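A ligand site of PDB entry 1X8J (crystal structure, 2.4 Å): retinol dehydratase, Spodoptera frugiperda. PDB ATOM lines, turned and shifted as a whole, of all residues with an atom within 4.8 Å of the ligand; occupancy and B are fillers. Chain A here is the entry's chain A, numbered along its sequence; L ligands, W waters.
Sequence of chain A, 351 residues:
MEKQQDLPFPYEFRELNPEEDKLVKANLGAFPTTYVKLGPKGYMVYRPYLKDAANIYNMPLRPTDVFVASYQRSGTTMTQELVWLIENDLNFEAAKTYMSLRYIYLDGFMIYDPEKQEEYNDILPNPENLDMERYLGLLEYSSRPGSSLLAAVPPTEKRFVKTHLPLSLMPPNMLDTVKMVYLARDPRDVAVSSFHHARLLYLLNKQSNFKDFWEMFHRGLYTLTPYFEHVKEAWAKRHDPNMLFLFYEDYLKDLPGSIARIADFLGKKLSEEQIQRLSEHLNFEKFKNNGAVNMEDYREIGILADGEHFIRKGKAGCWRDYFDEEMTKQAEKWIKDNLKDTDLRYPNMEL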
ATOM      1  N   SER A  70      30.665 -14.698  13.483  1.00  0.00           N
ATOM      2  CA  SER A  70      30.263 -14.323  12.135  1.00  0.00           C
ATOM      3  C   SER A  70      29.551 -12.999  12.169  1.00  0.00           C
ATOM      4  O   SER A  70      29.098 -12.543  13.223  1.00  0.00           O
ATOM      5  CB  SER A  70      29.242 -15.329  11.598  1.00  0.00           C
ATOM      6  OG  SER A  70      28.001 -15.154  12.275  1.00  0.00           O
ATOM      7  N   GLN A  72      26.241 -11.413  11.377  1.00  0.00           N
ATOM      8  CA  GLN A  72      24.909 -12.011  11.315  1.00  0.00           C
ATOM      9  C   GLN A  72      24.378 -12.431   9.949  1.00  0.00           C
ATOM     10  O   GLN A  72      24.659 -11.784   8.927  1.00  0.00           O
ATOM     11  CB  GLN A  72      23.896 -11.079  11.991  1.00  0.00           C
ATOM     12  CG  GLN A  72      23.733  -9.730  11.304  1.00  0.00           C
ATOM     13  CD  GLN A  72      22.446  -9.032  11.717  1.00  0.00           C
ATOM     14  OE1 GLN A  72      22.262  -8.701  12.888  1.00  0.00           O
ATOM     15  NE2 GLN A  72      21.554  -8.825  10.757  1.00  0.00           N
ATOM     16  N   ARG A  73      23.597 -13.512   9.945  1.00  0.00           N
ATOM     17  CA  ARG A  73      22.972 -14.063   8.741  1.00  0.00           C
ATOM     18  C   ARG A  73      23.974 -14.642   7.752  1.00  0.00           C
ATOM     19  O   ARG A  73      23.763 -14.587   6.535  1.00  0.00           O
ATOM     20  CB  ARG A  73      22.107 -12.979   8.055  1.00  0.00           C
ATOM     21  CG  ARG A  73      21.269 -12.167   9.027  1.00  0.00           C
ATOM     22  CD  ARG A  73      20.384 -13.078   9.838  1.00  0.00           C
ATOM     23  NE  ARG A  73      19.393 -13.731   8.998  1.00  0.00           N
ATOM     24  CZ  ARG A  73      18.669 -14.784   9.380  1.00  0.00           C
ATOM     25  NH1 ARG A  73      18.839 -15.309  10.580  1.00  0.00           N
ATOM     26  NH2 ARG A  73      17.768 -15.291   8.559  1.00  0.00           N
ATOM     27  N   SER A  74      25.053 -15.203   8.270  1.00  0.00           N
ATOM     28  CA  SER A  74      26.088 -15.782   7.412  1.00  0.00           C
ATOM     29  C   SER A  74      26.226 -17.282   7.566  1.00  0.00           C
ATOM     30  O   SER A  74      27.159 -17.874   7.023  1.00  0.00           O
ATOM     31  CB  SER A  74      27.437 -15.132   7.703  1.00  0.00           C
ATOM     32  OG  SER A  74      27.393 -13.735   7.507  1.00  0.00           O
ATOM     33  N   GLY A  75      25.326 -17.905   8.333  1.00  0.00           N
ATOM     34  CA  GLY A  75      25.403 -19.341   8.509  1.00  0.00           C
ATOM     35  C   GLY A  75      25.706 -19.757   9.941  1.00  0.00           C
ATOM     36  O   GLY A  75      26.070 -20.916  10.191  1.00  0.00           O
ATOM     37  N   THR A  76      25.524 -18.820  10.866  1.00  0.00           N
ATOM     38  CA  THR A  76      25.776 -19.082  12.292  1.00  0.00           C
ATOM     39  C   THR A  76      25.010 -20.282  12.835  1.00  0.00           C
ATOM     40  O   THR A  76      25.605 -21.238  13.327  1.00  0.00           O
ATOM     41  CB  THR A  76      25.386 -17.879  13.171  1.00  0.00           C
ATOM     42  OG1 THR A  76      25.909 -16.666  12.609  1.00  0.00           O
ATOM     43  CG2 THR A  76      25.942 -18.068  14.582  1.00  0.00           C
ATOM     44  N   THR A  77      23.673 -20.220  12.751  1.00  0.00           N
ATOM     45  CA  THR A  77      22.805 -21.277  13.263  1.00  0.00           C
ATOM     46  C   THR A  77      23.168 -22.684  12.784  1.00  0.00           C
ATOM     47  O   THR A  77      23.239 -23.616  13.598  1.00  0.00           O
ATOM     48  CB  THR A  77      21.325 -20.982  12.907  1.00  0.00           C
ATOM     49  OG1 THR A  77      21.016 -19.627  13.244  1.00  0.00           O
ATOM     50  CG2 THR A  77      20.390 -21.889  13.700  1.00  0.00           C
ATOM     51  N   MET A  78      23.374 -22.847  11.483  1.00  0.00           N
ATOM     52  CA  MET A  78      23.774 -24.146  10.919  1.00  0.00           C
ATOM     53  C   MET A  78      25.040 -24.625  11.596  1.00  0.00           C
ATOM     54  O   MET A  78      25.139 -25.762  12.049  1.00  0.00           O
ATOM     55  CB  MET A  78      24.131 -24.023   9.438  1.00  0.00           C
ATOM     56  CG  MET A  78      23.081 -23.455   8.554  1.00  0.00           C
ATOM     57  SD  MET A  78      23.752 -23.329   6.892  1.00  0.00           S
ATOM     58  CE  MET A  78      23.775 -25.092   6.452  1.00  0.00           C
ATOM     59  N   ARG A 185      29.852 -14.847   4.430  1.00  0.00           N
ATOM     60  CA  ARG A 185      28.921 -15.053   3.328  1.00  0.00           C
ATOM     61  C   ARG A 185      28.961 -13.823   2.397  1.00  0.00           C
ATOM     62  O   ARG A 185      29.382 -12.735   2.819  1.00  0.00           O
ATOM     63  CB  ARG A 185      27.511 -15.246   3.898  1.00  0.00           C
ATOM     64  CG  ARG A 185      26.421 -15.518   2.895  1.00  0.00           C
ATOM     65  CD  ARG A 185      25.048 -15.569   3.577  1.00  0.00           C
ATOM     66  NE  ARG A 185      24.025 -16.134   2.689  1.00  0.00           N
ATOM     67  CZ  ARG A 185      22.728 -16.182   2.969  1.00  0.00           C
ATOM     68  NH1 ARG A 185      22.265 -15.696   4.116  1.00  0.00           N
ATOM     69  NH2 ARG A 185      21.889 -16.752   2.104  1.00  0.00           N
ATOM     70  N   SER A 193      19.254 -11.069   3.666  1.00  0.00           N
ATOM     71  CA  SER A 193      18.861 -11.837   4.841  1.00  0.00           C
ATOM     72  C   SER A 193      18.714 -10.922   6.075  1.00  0.00           C
ATOM     73  O   SER A 193      17.788 -11.093   6.874  1.00  0.00           O
ATOM     74  CB  SER A 193      19.892 -12.937   5.125  1.00  0.00           C
ATOM     75  OG  SER A 193      19.456 -13.792   6.176  1.00  0.00           O
ATOM     76  N   TYR A 248      29.729 -19.523   3.892  1.00  0.00           N
ATOM     77  CA  TYR A 248      28.369 -20.049   3.893  1.00  0.00           C
ATOM     78  C   TYR A 248      28.093 -20.773   2.580  1.00  0.00           C
ATOM     79  O   TYR A 248      27.474 -21.837   2.577  1.00  0.00           O
ATOM     80  CB  TYR A 248      27.375 -18.903   4.072  1.00  0.00           C
ATOM     81  CG  TYR A 248      25.936 -19.309   3.825  1.00  0.00           C
ATOM     82  CD1 TYR A 248      25.204 -19.995   4.798  1.00  0.00           C
ATOM     83  CD2 TYR A 248      25.319 -19.033   2.613  1.00  0.00           C
ATOM     84  CE1 TYR A 248      23.895 -20.392   4.564  1.00  0.00           C
ATOM     85  CE2 TYR A 248      24.007 -19.433   2.370  1.00  0.00           C
ATOM     86  CZ  TYR A 248      23.305 -20.115   3.343  1.00  0.00           C
ATOM     87  OH  TYR A 248      22.011 -20.524   3.086  1.00  0.00           O
ATOM     88  N   LEU A 252      26.473 -25.040   0.891  1.00  0.00           N
ATOM     89  CA  LEU A 252      25.537 -25.376  -0.173  1.00  0.00           C
ATOM     90  C   LEU A 252      26.191 -26.223  -1.263  1.00  0.00           C
ATOM     91  O   LEU A 252      25.626 -27.217  -1.712  1.00  0.00           O
ATOM     92  CB  LEU A 252      24.960 -24.105  -0.791  1.00  0.00           C
ATOM     93  CG  LEU A 252      24.194 -23.181   0.160  1.00  0.00           C
ATOM     94  CD1 LEU A 252      23.808 -21.900  -0.561  1.00  0.00           C
ATOM     95  CD2 LEU A 252      22.945 -23.885   0.697  1.00  0.00           C
ATOM     96  N   LEU A 282      21.027 -31.495   8.521  1.00  0.00           N
ATOM     97  CA  LEU A 282      21.097 -30.081   8.167  1.00  0.00           C
ATOM     98  C   LEU A 282      20.344 -29.715   6.905  1.00  0.00           C
ATOM     99  O   LEU A 282      20.490 -28.598   6.385  1.00  0.00           O
ATOM    100  CB  LEU A 282      22.560 -29.643   8.062  1.00  0.00           C
ATOM    101  CG  LEU A 282      23.151 -28.982   9.310  1.00  0.00           C
ATOM    102  CD1 LEU A 282      22.533 -27.605   9.485  1.00  0.00           C
ATOM    103  CD2 LEU A 282      22.896 -29.853  10.539  1.00  0.00           C
ATOM    104  N   ASN A 283      19.530 -30.639   6.402  1.00  0.00           N
ATOM    105  CA  ASN A 283      18.718 -30.389   5.200  1.00  0.00           C
ATOM    106  C   ASN A 283      17.842 -29.159   5.482  1.00  0.00           C
ATOM    107  O   ASN A 283      17.151 -29.106   6.494  1.00  0.00           O
ATOM    108  CB  ASN A 283      17.868 -31.637   4.908  1.00  0.00           C
ATOM    109  CG  ASN A 283      16.880 -31.424   3.780  1.00  0.00           C
ATOM    110  OD1 ASN A 283      15.759 -30.968   4.006  1.00  0.00           O
ATOM    111  ND2 ASN A 283      17.278 -31.753   2.555  1.00  0.00           N
ATOM    112  N   PHE A 284      17.871 -28.170   4.590  1.00  0.00           N
ATOM    113  CA  PHE A 284      17.113 -26.938   4.803  1.00  0.00           C
ATOM    114  C   PHE A 284      15.652 -27.091   5.259  1.00  0.00           C
ATOM    115  O   PHE A 284      15.250 -26.482   6.256  1.00  0.00           O
ATOM    116  CB  PHE A 284      17.151 -26.041   3.567  1.00  0.00           C
ATOM    117  CG  PHE A 284      16.575 -24.665   3.805  1.00  0.00           C
ATOM    118  CD1 PHE A 284      17.288 -23.733   4.562  1.00  0.00           C
ATOM    119  CD2 PHE A 284      15.306 -24.338   3.344  1.00  0.00           C
ATOM    120  CE1 PHE A 284      16.740 -22.480   4.859  1.00  0.00           C
ATOM    121  CE2 PHE A 284      14.745 -23.085   3.645  1.00  0.00           C
ATOM    122  CZ  PHE A 284      15.466 -22.159   4.402  1.00  0.00           C
ATOM    123  N   PHE A 287      15.617 -28.667   8.707  1.00  0.00           N
ATOM    124  CA  PHE A 287      16.148 -27.727   9.689  1.00  0.00           C
ATOM    125  C   PHE A 287      15.160 -26.577   9.940  1.00  0.00           C
ATOM    126  O   PHE A 287      14.930 -26.190  11.088  1.00  0.00           O
ATOM    127  CB  PHE A 287      17.480 -27.174   9.191  1.00  0.00           C
ATOM    128  CG  PHE A 287      18.380 -26.668  10.272  1.00  0.00           C
ATOM    129  CD1 PHE A 287      18.797 -27.522  11.307  1.00  0.00           C
ATOM    130  CD2 PHE A 287      18.840 -25.360  10.264  1.00  0.00           C
ATOM    131  CE1 PHE A 287      19.648 -27.067  12.298  1.00  0.00           C
ATOM    132  CE2 PHE A 287      19.697 -24.897  11.252  1.00  0.00           C
ATOM    133  CZ  PHE A 287      20.106 -25.761  12.281  1.00  0.00           C
ATOM    134  N   PHE A 310      13.257 -17.191  10.933  1.00  0.00           N
ATOM    135  CA  PHE A 310      14.693 -17.134  11.159  1.00  0.00           C
ATOM    136  C   PHE A 310      15.383 -17.909  10.048  1.00  0.00           C
ATOM    137  O   PHE A 310      16.378 -17.447   9.504  1.00  0.00           O
ATOM    138  CB  PHE A 310      15.079 -17.723  12.507  1.00  0.00           C
ATOM    139  CG  PHE A 310      14.889 -16.778  13.648  1.00  0.00           C
ATOM    140  CD1 PHE A 310      13.653 -16.702  14.308  1.00  0.00           C
ATOM    141  CD2 PHE A 310      15.944 -15.986  14.106  1.00  0.00           C
ATOM    142  CE1 PHE A 310      13.473 -15.832  15.402  1.00  0.00           C
ATOM    143  CE2 PHE A 310      15.785 -15.123  15.196  1.00  0.00           C
ATOM    144  CZ  PHE A 310      14.533 -15.050  15.850  1.00  0.00           C
ATOM    145  N   ILE A 311      14.858 -19.090   9.737  1.00  0.00           N
ATOM    146  CA  ILE A 311      15.382 -19.950   8.678  1.00  0.00           C
ATOM    147  C   ILE A 311      14.464 -19.655   7.496  1.00  0.00           C
ATOM    148  O   ILE A 311      13.335 -20.131   7.458  1.00  0.00           O
ATOM    149  CB  ILE A 311      15.302 -21.411   9.114  1.00  0.00           C
ATOM    150  CG1 ILE A 311      16.092 -21.587  10.419  1.00  0.00           C
ATOM    151  CG2 ILE A 311      15.852 -22.317   8.038  1.00  0.00           C
ATOM    152  CD1 ILE A 311      15.952 -22.946  11.081  1.00  0.00           C
ATOM    153  N   ARG A 312      14.963 -18.856   6.550  1.00  0.00           N
ATOM    154  CA  ARG A 312      14.176 -18.399   5.402  1.00  0.00           C
ATOM    155  C   ARG A 312      14.166 -19.184   4.081  1.00  0.00           C
ATOM    156  O   ARG A 312      13.327 -20.063   3.886  1.00  0.00           O
ATOM    157  CB  ARG A 312      14.575 -16.948   5.113  1.00  0.00           C
ATOM    158  CG  ARG A 312      13.540 -16.101   4.404  1.00  0.00           C
ATOM    159  CD  ARG A 312      13.949 -14.643   4.488  1.00  0.00           C
ATOM    160  NE  ARG A 312      15.290 -14.440   3.934  1.00  0.00           N
ATOM    161  CZ  ARG A 312      15.561 -14.348   2.629  1.00  0.00           C
ATOM    162  NH1 ARG A 312      14.582 -14.425   1.742  1.00  0.00           N
ATOM    163  NH2 ARG A 312      16.814 -14.176   2.219  1.00  0.00           N
ATOM    164  N   LYS A 313      15.071 -18.834   3.183  1.00  0.00           N
ATOM    165  CA  LYS A 313      15.169 -19.452   1.869  1.00  0.00           C
ATOM    166  C   LYS A 313      16.352 -20.420   1.769  1.00  0.00           C
ATOM    167  O   LYS A 313      16.274 -21.437   1.073  1.00  0.00           O
ATOM    168  CB  LYS A 313      15.320 -18.361   0.804  1.00  0.00           C
ATOM    169  CG  LYS A 313      14.101 -18.163  -0.110  1.00  0.00           C
ATOM    170  CD  LYS A 313      14.136 -19.116  -1.300  1.00  0.00           C
ATOM    171  CE  LYS A 313      13.282 -18.598  -2.467  1.00  0.00           C
ATOM    172  NZ  LYS A 313      11.850 -18.366  -2.096  1.00  0.00           N
ATOM    173  N   GLY A 314      17.454 -20.102   2.453  1.00  0.00           N
ATOM    174  CA  GLY A 314      18.618 -20.960   2.446  1.00  0.00           C
ATOM    175  C   GLY A 314      19.298 -21.143   1.096  1.00  0.00           C
ATOM    176  O   GLY A 314      19.802 -22.219   0.795  1.00  0.00           O
ATOM    177  N   LYS A 315      19.326 -20.085   0.304  1.00  0.00           N
ATOM    178  CA  LYS A 315      19.927 -20.117  -1.022  1.00  0.00           C
ATOM    179  C   LYS A 315      21.057 -19.101  -1.169  1.00  0.00           C
ATOM    180  O   LYS A 315      21.189 -18.181  -0.354  1.00  0.00           O
ATOM    181  CB  LYS A 315      18.867 -19.822  -2.087  1.00  0.00           C
ATOM    182  CG  LYS A 315      17.678 -20.777  -2.081  1.00  0.00           C
ATOM    183  CD  LYS A 315      18.069 -22.185  -2.492  1.00  0.00           C
ATOM    184  CE  LYS A 315      16.828 -23.085  -2.626  1.00  0.00           C
ATOM    185  NZ  LYS A 315      17.174 -24.467  -3.086  1.00  0.00           N
HETATM  186  P1  LIG L   1      18.607 -16.560   4.139  1.00  0.00           P
HETATM  187  O1  LIG L   1      19.267 -16.212   2.872  1.00  0.00           O
HETATM  188  O2  LIG L   1      17.623 -17.617   3.908  1.00  0.00           O
HETATM  189  O3  LIG L   1      17.993 -15.371   4.765  1.00  0.00           O
HETATM  190  P2  LIG L   1      22.480 -17.021  10.606  1.00  0.00           P
HETATM  191  O4  LIG L   1      23.920 -16.788  10.717  1.00  0.00           O
HETATM  192  O5  LIG L   1      22.131 -18.300  11.242  1.00  0.00           O
HETATM  193  O6  LIG L   1      21.710 -15.901  11.200  1.00  0.00           O
HETATM  194  O7  LIG L   1      22.125 -17.112   9.073  1.00  0.00           O
HETATM  195  C1  LIG L   1      20.802 -17.301   8.623  1.00  0.00           C
HETATM  196  C2  LIG L   1      20.833 -17.698   7.137  1.00  0.00           C
HETATM  197  O8  LIG L   1      21.211 -19.109   7.043  1.00  0.00           O
HETATM  198  C3  LIG L   1      19.485 -17.584   6.468  1.00  0.00           C
HETATM  199  O9  LIG L   1      19.713 -17.131   5.106  1.00  0.00           O
HETATM  200  C4  LIG L   1      18.932 -19.009   6.666  1.00  0.00           C
HETATM  201  O10 LIG L   1      17.773 -19.404   5.933  1.00  0.00           O
HETATM  202  C5  LIG L   1      20.173 -19.824   6.386  1.00  0.00           C
HETATM  203  N1  LIG L   1      20.072 -21.194   6.931  1.00  0.00           N
HETATM  204  C6  LIG L   1      19.704 -21.621   8.198  1.00  0.00           C
HETATM  205  N2  LIG L   1      19.714 -22.919   8.366  1.00  0.00           N
HETATM  206  C7  LIG L   1      20.120 -23.404   7.129  1.00  0.00           C
HETATM  207  C8  LIG L   1      20.345 -24.737   6.594  1.00  0.00           C
HETATM  208  N3  LIG L   1      20.178 -25.873   7.309  1.00  0.00           N
HETATM  209  N4  LIG L   1      20.761 -24.842   5.258  1.00  0.00           N
HETATM  210  C9  LIG L   1      20.946 -23.729   4.500  1.00  0.00           C
HETATM  211  N5  LIG L   1      20.759 -22.435   4.894  1.00  0.00           N
HETATM  212  C10 LIG L   1      20.349 -22.338   6.220  1.00  0.00           C
HETATM  213  O   HOH W   1      16.172 -13.366   6.947  1.00  0.00           O
HETATM  214  O   HOH W   2      22.461 -20.761   9.752  1.00  0.00           O
HETATM  215  O   HOH W   3      19.827 -13.944   1.235  1.00  0.00           O
HETATM  216  O   HOH W   4      18.464 -17.203   0.537  1.00  0.00           O
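OG of Ser 193 sits at hydrogen-bond distance from NE of Arg 73 (2.8 Å).
The side-chain hydroxyl of Thr 76 is in hydrogen-bond range of the side-chain hydroxyl of Ser 70 (2.6 Å).
NH1 of Arg 185 is in hydrogen-bond range of O of Arg 73.
The backbone carbonyl oxygen (O) of Lys 315 sits at hydrogen-bond distance from the guanidinium group (NH2) of Arg 185 (2.9 Å).
The guanidinium group of Arg 73 sits at hydrogen-bond distance from the backbone carbonyl oxygen of Phe 310 (2.7 Å).
Water W4 bridges O1 of the ligand (2.7 Å) and N of Lys 315 (3.0 Å).
Water W3 lies within hydrogen-bond range of an oxygen (O1) of the ligand (2.9 Å) and the guanidinium group (NH2) of Arg 312 (3.2 Å).
Water W2 lies within hydrogen-bond range of the backbone NH (N) of Met 78 (2.9 Å), an oxygen (O5) of the ligand (2.9 Å) and the backbone NH (N) of Thr 77 (3.3 Å).
Water W1 lies within hydrogen-bond range of the backbone carbonyl oxygen of Ser 193 (2.8 Å), the guanidinium group of Arg 73 (3.0 Å), the guanidinium group of Arg 312 (3.3 Å) and an oxygen (O3) of the ligand (3.5 Å).
O3 of the ligand sits at hydrogen-bond distance from OG of Ser 193.
N of Thr 76 sits at hydrogen-bond distance from O4 of the ligand, 2.6 Å away.
An oxygen (O4) of the ligand lies within hydrogen-bond range of the side-chain hydroxyl (OG1) of Thr 76 (2.7 Å).
N of Thr 77 lies within hydrogen-bond range of O5 of the ligand, 2.9 Å away.
An oxygen (O5) of the ligand is in hydrogen-bond range of the side-chain hydroxyl (OG1) of Thr 77.
NH2 of Arg 185 lies within salt-bridge range of O1 of the ligand (2.8 Å).
N of Gly 314 lies within hydrogen-bond range of O2 of the ligand, 2.9 Å away.
A nitrogen (N3) of the ligand sits at hydrogen-bond distance from the backbone carbonyl oxygen (O) of Leu 282, at 2.9 Å.
OH of Tyr 248 lies within hydrogen-bond range of N5 of the ligand.
The backbone NH (N) of Lys 313 lies within hydrogen-bond range of an oxygen (O2) of the ligand (2.9 Å).
The backbone NH (N) of Arg 312 lies within hydrogen-bond range of an oxygen (O10) of the ligand (2.9 Å).
The guanidinium group of Arg 312 is in salt-bridge range of an oxygen (O3) of the ligand.
The backbone NH (N) of Gly 75 sits at hydrogen-bond distance from an oxygen (O4) of the ligand (3.0 Å).
O6 of the ligand lies within hydrogen-bond range of N of Arg 73 (3.3 Å).
An oxygen (O6) of the ligand is in salt-bridge range of the guanidinium group (NH1) of Arg 73.
The backbone NH of Ser 74 lies within hydrogen-bond range of an oxygen (O4) of the ligand (3.1 Å).
SD of Met 78 lies close to N5 of the ligand (3.7 Å).
Residues that only touch the ligand: Phe 287, Phe 284 and Ile 311.
Hydrophobic or aromatic side chains within 4 Å of the ligand: Met 78, Tyr 248, Leu 282, Phe 284, Phe 287 and Ile 311.
16 residues have an atom within 4 Å of the ligand: Arg 73, Ser 74, Gly 75, Thr 76, Thr 77, Met 78, Arg 185, Ser 193, Tyr 248, Leu 282, Phe 284, Phe 287, Ile 311, Arg 312, Lys 313 and Gly 314.
The nearest printed residue that does not touch the ligand is Phe 310 (4.1 Å).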
